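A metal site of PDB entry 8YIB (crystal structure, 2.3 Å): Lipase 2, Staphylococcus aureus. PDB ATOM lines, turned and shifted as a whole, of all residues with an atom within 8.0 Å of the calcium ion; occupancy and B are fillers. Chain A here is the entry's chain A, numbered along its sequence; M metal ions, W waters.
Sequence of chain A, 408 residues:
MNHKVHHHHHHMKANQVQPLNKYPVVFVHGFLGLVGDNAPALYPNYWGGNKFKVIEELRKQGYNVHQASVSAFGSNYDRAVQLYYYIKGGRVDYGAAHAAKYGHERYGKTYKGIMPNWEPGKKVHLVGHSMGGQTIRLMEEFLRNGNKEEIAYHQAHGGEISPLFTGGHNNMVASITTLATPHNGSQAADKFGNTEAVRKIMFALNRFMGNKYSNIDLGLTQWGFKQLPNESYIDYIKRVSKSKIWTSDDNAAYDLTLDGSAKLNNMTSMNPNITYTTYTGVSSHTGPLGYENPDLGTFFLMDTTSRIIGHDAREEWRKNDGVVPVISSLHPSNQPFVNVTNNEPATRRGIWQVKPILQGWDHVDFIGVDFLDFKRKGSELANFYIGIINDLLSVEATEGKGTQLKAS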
ATOM      1  N   LYS A  51     -26.102 -18.344  21.965  1.00  0.00           N
ATOM      2  CA  LYS A  51     -26.732 -19.250  21.013  1.00  0.00           C
ATOM      3  C   LYS A  51     -28.239 -19.058  20.994  1.00  0.00           C
ATOM      4  O   LYS A  51     -28.826 -19.047  19.929  1.00  0.00           O
ATOM      5  CB  LYS A  51     -26.285 -20.685  21.296  1.00  0.00           C
ATOM      6  CG  LYS A  51     -24.823 -20.933  20.960  1.00  0.00           C
ATOM      7  CD  LYS A  51     -24.446 -22.387  20.982  1.00  0.00           C
ATOM      8  CE  LYS A  51     -22.968 -22.604  20.770  1.00  0.00           C
ATOM      9  NZ  LYS A  51     -22.626 -24.048  20.867  1.00  0.00           N
ATOM     10  N   SER A 283     -21.348 -37.178  26.399  1.00  0.00           N
ATOM     11  CA  SER A 283     -20.351 -36.525  25.575  1.00  0.00           C
ATOM     12  C   SER A 283     -19.030 -37.276  25.735  1.00  0.00           C
ATOM     13  O   SER A 283     -17.940 -36.700  25.572  1.00  0.00           O
ATOM     14  CB  SER A 283     -20.227 -35.058  25.957  1.00  0.00           C
ATOM     15  OG  SER A 283     -19.285 -34.383  25.133  1.00  0.00           O
ATOM     16  N   ASP A 295     -15.547 -36.832  24.259  1.00  0.00           N
ATOM     17  CA  ASP A 295     -15.572 -36.480  22.846  1.00  0.00           C
ATOM     18  C   ASP A 295     -14.866 -35.144  22.634  1.00  0.00           C
ATOM     19  O   ASP A 295     -14.908 -34.267  23.501  1.00  0.00           O
ATOM     20  CB  ASP A 295     -17.013 -36.330  22.354  1.00  0.00           C
ATOM     21  CG  ASP A 295     -17.860 -37.579  22.449  1.00  0.00           C
ATOM     22  OD1 ASP A 295     -17.279 -38.669  22.794  1.00  0.00           O
ATOM     23  OD2 ASP A 295     -19.093 -37.471  22.186  1.00  0.00           O
ATOM     24  N   LEU A 296     -14.195 -35.006  21.475  1.00  0.00           N
ATOM     25  CA  LEU A 296     -13.919 -33.709  20.870  1.00  0.00           C
ATOM     26  C   LEU A 296     -15.215 -32.925  20.951  1.00  0.00           C
ATOM     27  O   LEU A 296     -16.264 -33.441  20.546  1.00  0.00           O
ATOM     28  CB  LEU A 296     -13.587 -33.960  19.389  1.00  0.00           C
ATOM     29  CG  LEU A 296     -12.142 -34.233  18.952  1.00  0.00           C
ATOM     30  CD1 LEU A 296     -11.282 -34.881  20.035  1.00  0.00           C
ATOM     31  CD2 LEU A 296     -12.144 -35.130  17.710  1.00  0.00           C
ATOM     32  N   GLY A 297     -15.189 -31.701  21.477  1.00  0.00           N
ATOM     33  CA  GLY A 297     -16.461 -31.001  21.495  1.00  0.00           C
ATOM     34  C   GLY A 297     -17.062 -30.875  22.897  1.00  0.00           C
ATOM     35  O   GLY A 297     -17.922 -30.041  23.144  1.00  0.00           O
ATOM     36  N   THR A 298     -16.618 -31.751  23.801  1.00  0.00           N
ATOM     37  CA  THR A 298     -16.751 -31.494  25.215  1.00  0.00           C
ATOM     38  C   THR A 298     -16.010 -30.193  25.491  1.00  0.00           C
ATOM     39  O   THR A 298     -14.831 -30.068  25.158  1.00  0.00           O
ATOM     40  CB  THR A 298     -16.053 -32.592  26.035  1.00  0.00           C
ATOM     41  OG1 THR A 298     -16.484 -33.873  25.574  1.00  0.00           O
ATOM     42  CG2 THR A 298     -16.325 -32.480  27.521  1.00  0.00           C
ATOM     43  N   PHE A 299     -16.725 -29.197  26.038  1.00  0.00           N
ATOM     44  CA  PHE A 299     -16.058 -27.976  26.453  1.00  0.00           C
ATOM     45  C   PHE A 299     -14.784 -28.302  27.266  1.00  0.00           C
ATOM     46  O   PHE A 299     -14.832 -29.078  28.223  1.00  0.00           O
ATOM     47  CB  PHE A 299     -17.022 -27.110  27.243  1.00  0.00           C
ATOM     48  CG  PHE A 299     -16.500 -25.727  27.494  1.00  0.00           C
ATOM     49  CD1 PHE A 299     -16.273 -24.850  26.439  1.00  0.00           C
ATOM     50  CD2 PHE A 299     -16.228 -25.307  28.790  1.00  0.00           C
ATOM     51  CE1 PHE A 299     -15.794 -23.580  26.675  1.00  0.00           C
ATOM     52  CE2 PHE A 299     -15.734 -24.029  29.025  1.00  0.00           C
ATOM     53  CZ  PHE A 299     -15.511 -23.172  27.965  1.00  0.00           C
ATOM     54  N   PHE A 300     -13.651 -27.702  26.865  1.00  0.00           N
ATOM     55  CA  PHE A 300     -12.317 -28.191  27.241  1.00  0.00           C
ATOM     56  C   PHE A 300     -12.085 -28.146  28.747  1.00  0.00           C
ATOM     57  O   PHE A 300     -11.286 -28.925  29.272  1.00  0.00           O
ATOM     58  CB  PHE A 300     -11.185 -27.423  26.522  1.00  0.00           C
ATOM     59  CG  PHE A 300     -11.012 -25.989  26.961  1.00  0.00           C
ATOM     60  CD1 PHE A 300     -11.876 -24.996  26.518  1.00  0.00           C
ATOM     61  CD2 PHE A 300     -10.006 -25.641  27.861  1.00  0.00           C
ATOM     62  CE1 PHE A 300     -11.742 -23.670  26.957  1.00  0.00           C
ATOM     63  CE2 PHE A 300      -9.874 -24.325  28.298  1.00  0.00           C
ATOM     64  CZ  PHE A 300     -10.735 -23.340  27.844  1.00  0.00           C
ATOM     65  N   MET A 302     -13.798 -29.333  30.899  1.00  0.00           N
ATOM     66  CA  MET A 302     -14.366 -30.522  31.527  1.00  0.00           C
ATOM     67  C   MET A 302     -13.596 -31.788  31.144  1.00  0.00           C
ATOM     68  O   MET A 302     -13.959 -32.901  31.531  1.00  0.00           O
ATOM     69  CB  MET A 302     -15.839 -30.678  31.122  1.00  0.00           C
ATOM     70  CG  MET A 302     -16.715 -29.755  31.906  1.00  0.00           C
ATOM     71  SD  MET A 302     -18.456 -30.031  31.535  1.00  0.00           S
ATOM     72  CE  MET A 302     -18.533 -29.704  29.776  1.00  0.00           C
ATOM     73  N   ASP A 321     -21.411 -36.493  30.844  1.00  0.00           N
ATOM     74  CA  ASP A 321     -21.640 -35.291  30.058  1.00  0.00           C
ATOM     75  C   ASP A 321     -20.466 -34.300  30.198  1.00  0.00           C
ATOM     76  O   ASP A 321     -20.604 -33.121  29.843  1.00  0.00           O
ATOM     77  CB  ASP A 321     -22.959 -34.611  30.434  1.00  0.00           C
ATOM     78  CG  ASP A 321     -22.903 -33.851  31.765  1.00  0.00           C
ATOM     79  OD1 ASP A 321     -21.828 -33.873  32.438  1.00  0.00           O
ATOM     80  OD2 ASP A 321     -23.928 -33.215  32.111  1.00  0.00           O
ATOM     81  N   GLY A 360     -24.019 -36.351  22.220  1.00  0.00           N
ATOM     82  CA  GLY A 360     -23.105 -35.264  21.901  1.00  0.00           C
ATOM     83  C   GLY A 360     -23.298 -33.983  22.743  1.00  0.00           C
ATOM     84  O   GLY A 360     -22.530 -33.032  22.605  1.00  0.00           O
ATOM     85  N   TRP A 361     -24.323 -33.948  23.605  1.00  0.00           N
ATOM     86  CA  TRP A 361     -24.563 -32.772  24.442  1.00  0.00           C
ATOM     87  C   TRP A 361     -23.773 -32.900  25.739  1.00  0.00           C
ATOM     88  O   TRP A 361     -24.072 -33.778  26.547  1.00  0.00           O
ATOM     89  CB  TRP A 361     -26.057 -32.663  24.769  1.00  0.00           C
ATOM     90  CG  TRP A 361     -26.933 -32.132  23.665  1.00  0.00           C
ATOM     91  CD1 TRP A 361     -26.947 -32.542  22.368  1.00  0.00           C
ATOM     92  CD2 TRP A 361     -27.971 -31.131  23.799  1.00  0.00           C
ATOM     93  NE1 TRP A 361     -27.917 -31.847  21.678  1.00  0.00           N
ATOM     94  CE2 TRP A 361     -28.571 -30.986  22.528  1.00  0.00           C
ATOM     95  CE3 TRP A 361     -28.439 -30.336  24.861  1.00  0.00           C
ATOM     96  CZ2 TRP A 361     -29.607 -30.087  22.287  1.00  0.00           C
ATOM     97  CZ3 TRP A 361     -29.485 -29.457  24.624  1.00  0.00           C
ATOM     98  CH2 TRP A 361     -30.051 -29.328  23.350  1.00  0.00           C
ATOM     99  N   ASP A 362     -22.747 -32.038  25.935  1.00  0.00           N
ATOM    100  CA  ASP A 362     -22.073 -32.014  27.225  1.00  0.00           C
ATOM    101  C   ASP A 362     -22.893 -31.181  28.212  1.00  0.00           C
ATOM    102  O   ASP A 362     -23.903 -30.565  27.856  1.00  0.00           O
ATOM    103  CB  ASP A 362     -20.628 -31.526  27.122  1.00  0.00           C
ATOM    104  CG  ASP A 362     -20.455 -30.077  26.677  1.00  0.00           C
ATOM    105  OD1 ASP A 362     -21.264 -29.203  27.111  1.00  0.00           O
ATOM    106  OD2 ASP A 362     -19.482 -29.816  25.939  1.00  0.00           O
ATOM    107  N   HIS A 363     -22.389 -31.141  29.444  1.00  0.00           N
ATOM    108  CA  HIS A 363     -23.020 -30.441  30.566  1.00  0.00           C
ATOM    109  C   HIS A 363     -23.419 -29.004  30.232  1.00  0.00           C
ATOM    110  O   HIS A 363     -24.478 -28.561  30.674  1.00  0.00           O
ATOM    111  CB  HIS A 363     -22.055 -30.446  31.765  1.00  0.00           C
ATOM    112  CG  HIS A 363     -22.727 -30.151  33.045  1.00  0.00           C
ATOM    113  ND1 HIS A 363     -23.628 -31.029  33.624  1.00  0.00           N
ATOM    114  CD2 HIS A 363     -22.626 -29.105  33.867  1.00  0.00           C
ATOM    115  CE1 HIS A 363     -24.065 -30.499  34.758  1.00  0.00           C
ATOM    116  NE2 HIS A 363     -23.461 -29.336  34.939  1.00  0.00           N
ATOM    117  N   VAL A 364     -22.570 -28.274  29.482  1.00  0.00           N
ATOM    118  CA  VAL A 364     -22.863 -26.863  29.257  1.00  0.00           C
ATOM    119  C   VAL A 364     -23.536 -26.649  27.889  1.00  0.00           C
ATOM    120  O   VAL A 364     -24.024 -25.547  27.636  1.00  0.00           O
ATOM    121  CB  VAL A 364     -21.660 -25.914  29.462  1.00  0.00           C
ATOM    122  CG1 VAL A 364     -21.104 -25.970  30.883  1.00  0.00           C
ATOM    123  CG2 VAL A 364     -20.555 -26.119  28.447  1.00  0.00           C
ATOM    124  N   ASP A 365     -23.597 -27.676  27.036  1.00  0.00           N
ATOM    125  CA  ASP A 365     -24.366 -27.505  25.806  1.00  0.00           C
ATOM    126  C   ASP A 365     -25.829 -27.216  26.146  1.00  0.00           C
ATOM    127  O   ASP A 365     -26.515 -26.545  25.397  1.00  0.00           O
ATOM    128  CB  ASP A 365     -24.187 -28.657  24.830  1.00  0.00           C
ATOM    129  CG  ASP A 365     -22.757 -28.810  24.294  1.00  0.00           C
ATOM    130  OD1 ASP A 365     -22.150 -27.767  23.902  1.00  0.00           O
ATOM    131  OD2 ASP A 365     -22.261 -29.956  24.231  1.00  0.00           O
ATOM    132  N   PHE A 366     -26.301 -27.710  27.305  1.00  0.00           N
ATOM    133  CA  PHE A 366     -27.686 -27.514  27.704  1.00  0.00           C
ATOM    134  C   PHE A 366     -28.027 -26.039  27.881  1.00  0.00           C
ATOM    135  O   PHE A 366     -29.199 -25.668  27.782  1.00  0.00           O
ATOM    136  CB  PHE A 366     -28.006 -28.270  28.999  1.00  0.00           C
ATOM    137  CG  PHE A 366     -28.223 -29.743  28.771  1.00  0.00           C
ATOM    138  CD1 PHE A 366     -29.476 -30.216  28.411  1.00  0.00           C
ATOM    139  CD2 PHE A 366     -27.166 -30.644  28.868  1.00  0.00           C
ATOM    140  CE1 PHE A 366     -29.684 -31.574  28.175  1.00  0.00           C
ATOM    141  CE2 PHE A 366     -27.370 -31.996  28.648  1.00  0.00           C
ATOM    142  CZ  PHE A 366     -28.626 -32.460  28.297  1.00  0.00           C
ATOM    143  N   VAL A 369     -23.452 -22.309  26.334  1.00  0.00           N
ATOM    144  CA  VAL A 369     -22.286 -21.469  26.591  1.00  0.00           C
ATOM    145  C   VAL A 369     -21.041 -22.090  25.983  1.00  0.00           C
ATOM    146  O   VAL A 369     -19.960 -21.538  26.156  1.00  0.00           O
ATOM    147  CB  VAL A 369     -22.070 -21.146  28.084  1.00  0.00           C
ATOM    148  CG1 VAL A 369     -23.262 -20.420  28.689  1.00  0.00           C
ATOM    149  CG2 VAL A 369     -21.737 -22.378  28.905  1.00  0.00           C
ATOM    150  N   ASP A 370     -21.162 -23.221  25.275  1.00  0.00           N
ATOM    151  CA  ASP A 370     -19.979 -23.803  24.689  1.00  0.00           C
ATOM    152  C   ASP A 370     -19.717 -23.119  23.347  1.00  0.00           C
ATOM    153  O   ASP A 370     -20.115 -23.632  22.299  1.00  0.00           O
ATOM    154  CB  ASP A 370     -20.094 -25.313  24.531  1.00  0.00           C
ATOM    155  CG  ASP A 370     -18.848 -25.974  23.957  1.00  0.00           C
ATOM    156  OD1 ASP A 370     -17.958 -25.243  23.482  1.00  0.00           O
ATOM    157  OD2 ASP A 370     -18.748 -27.216  24.035  1.00  0.00           O
ATOM    158  N   PHE A 371     -19.018 -21.967  23.398  1.00  0.00           N
ATOM    159  CA  PHE A 371     -18.814 -21.132  22.224  1.00  0.00           C
ATOM    160  C   PHE A 371     -17.851 -21.833  21.263  1.00  0.00           C
ATOM    161  O   PHE A 371     -17.786 -21.463  20.100  1.00  0.00           O
ATOM    162  CB  PHE A 371     -18.310 -19.728  22.587  1.00  0.00           C
ATOM    163  CG  PHE A 371     -16.962 -19.706  23.273  1.00  0.00           C
ATOM    164  CD1 PHE A 371     -16.858 -19.835  24.650  1.00  0.00           C
ATOM    165  CD2 PHE A 371     -15.789 -19.613  22.540  1.00  0.00           C
ATOM    166  CE1 PHE A 371     -15.617 -19.861  25.281  1.00  0.00           C
ATOM    167  CE2 PHE A 371     -14.546 -19.629  23.173  1.00  0.00           C
ATOM    168  CZ  PHE A 371     -14.470 -19.751  24.542  1.00  0.00           C
ATOM    169  N   LEU A 372     -17.103 -22.832  21.746  1.00  0.00           N
ATOM    170  CA  LEU A 372     -16.173 -23.575  20.906  1.00  0.00           C
ATOM    171  C   LEU A 372     -16.849 -24.688  20.076  1.00  0.00           C
ATOM    172  O   LEU A 372     -16.173 -25.320  19.299  1.00  0.00           O
ATOM    173  CB  LEU A 372     -15.106 -24.231  21.790  1.00  0.00           C
ATOM    174  CG  LEU A 372     -13.830 -23.446  22.096  1.00  0.00           C
ATOM    175  CD1 LEU A 372     -13.677 -22.192  21.241  1.00  0.00           C
ATOM    176  CD2 LEU A 372     -13.659 -23.163  23.579  1.00  0.00           C
ATOM    177  N   ASP A 373     -18.142 -24.977  20.267  1.00  0.00           N
ATOM    178  CA  ASP A 373     -18.695 -26.210  19.712  1.00  0.00           C
ATOM    179  C   ASP A 373     -19.694 -25.880  18.590  1.00  0.00           C
ATOM    180  O   ASP A 373     -20.834 -25.509  18.870  1.00  0.00           O
ATOM    181  CB  ASP A 373     -19.303 -27.100  20.803  1.00  0.00           C
ATOM    182  CG  ASP A 373     -19.822 -28.476  20.383  1.00  0.00           C
ATOM    183  OD1 ASP A 373     -19.875 -28.771  19.166  1.00  0.00           O
ATOM    184  OD2 ASP A 373     -20.161 -29.262  21.281  1.00  0.00           O
ATOM    185  N   PHE A 374     -19.277 -26.065  17.335  1.00  0.00           N
ATOM    186  CA  PHE A 374     -20.073 -25.599  16.209  1.00  0.00           C
ATOM    187  C   PHE A 374     -21.158 -26.607  15.835  1.00  0.00           C
ATOM    188  O   PHE A 374     -22.117 -26.232  15.163  1.00  0.00           O
ATOM    189  CB  PHE A 374     -19.200 -25.074  15.053  1.00  0.00           C
ATOM    190  CG  PHE A 374     -19.895 -24.126  14.112  1.00  0.00           C
ATOM    191  CD1 PHE A 374     -20.390 -22.900  14.551  1.00  0.00           C
ATOM    192  CD2 PHE A 374     -20.087 -24.448  12.770  1.00  0.00           C
ATOM    193  CE1 PHE A 374     -21.049 -22.038  13.678  1.00  0.00           C
ATOM    194  CE2 PHE A 374     -20.738 -23.589  11.902  1.00  0.00           C
ATOM    195  CZ  PHE A 374     -21.211 -22.381  12.356  1.00  0.00           C
ATOM    196  N   LYS A 375     -21.074 -27.848  16.331  1.00  0.00           N
ATOM    197  CA  LYS A 375     -22.119 -28.839  16.074  1.00  0.00           C
ATOM    198  C   LYS A 375     -23.406 -28.483  16.826  1.00  0.00           C
ATOM    199  O   LYS A 375     -24.494 -28.940  16.472  1.00  0.00           O
ATOM    200  CB  LYS A 375     -21.698 -30.281  16.411  1.00  0.00           C
ATOM    201  CG  LYS A 375     -20.316 -30.761  15.974  1.00  0.00           C
ATOM    202  CD  LYS A 375     -20.270 -32.228  15.529  1.00  0.00           C
ATOM    203  CE  LYS A 375     -20.847 -32.425  14.133  1.00  0.00           C
ATOM    204  NZ  LYS A 375     -20.805 -33.830  13.653  1.00  0.00           N
ATOM    205  N   ARG A 376     -23.303 -27.707  17.909  1.00  0.00           N
ATOM    206  CA  ARG A 376     -24.474 -27.432  18.724  1.00  0.00           C
ATOM    207  C   ARG A 376     -24.983 -26.020  18.371  1.00  0.00           C
ATOM    208  O   ARG A 376     -24.451 -25.033  18.879  1.00  0.00           O
ATOM    209  CB  ARG A 376     -24.123 -27.575  20.213  1.00  0.00           C
ATOM    210  CG  ARG A 376     -23.574 -28.946  20.623  1.00  0.00           C
ATOM    211  CD  ARG A 376     -24.675 -29.928  21.014  1.00  0.00           C
ATOM    212  NE  ARG A 376     -25.573 -30.355  19.950  1.00  0.00           N
ATOM    213  CZ  ARG A 376     -25.318 -31.321  19.055  1.00  0.00           C
ATOM    214  NH1 ARG A 376     -26.233 -31.684  18.181  1.00  0.00           N
ATOM    215  NH2 ARG A 376     -24.166 -31.967  19.092  1.00  0.00           N
HETATM  216 CA    CA M   1     -20.029 -29.285  23.717  1.00  0.00          CA
HETATM  217  O   HOH W   1     -20.096 -31.922  23.499  1.00  0.00           O
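Water W1 lies within hydrogen-bond range of the backbone carbonyl oxygen (O) of Gly 360 (2.8 Å), the side-chain hydroxyl (OG) of Ser 283 (3.1 Å) and the backbone NH (N) of Thr 298 (3.5 Å).
The calcium ion is bound by O of Gly 297 (2.3 Å), OD2 of Asp 362 (2.3 Å), OD2 of Asp 365 (2.4 Å), OD2 of Asp 373 (2.4 Å), OD2 of Asp 370 (2.5 Å), OD1 of Asp 365 (2.6 Å) and water W1 (2.6 Å). The calcium ion has seven donor atoms within binding distance.
The backbone NH (N) of Phe 299 lies close to the side-chain carboxylate (OD2) of Asp 362, 2.8 Å away. OD1 of Asp 362 sits at hydrogen-bond distance from N of Val 364, 2.9 Å away. The backbone carbonyl oxygen (O) of Asp 373 lies within hydrogen-bond range of the side-chain amino group (NZ) of Lys 51 (3.1 Å). OD1 of Asp 373 sits at hydrogen-bond distance from N of Lys 375, 3.2 Å away. OD2 of Asp 370 lies close to N of Phe 299. O of Asp 370 is in hydrogen-bond range of NZ of Lys 51, 2.9 Å away. The backbone NH (N) of Leu 372 sits close to the side-chain carboxylate (OD1) of Asp 370 (3.1 Å).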
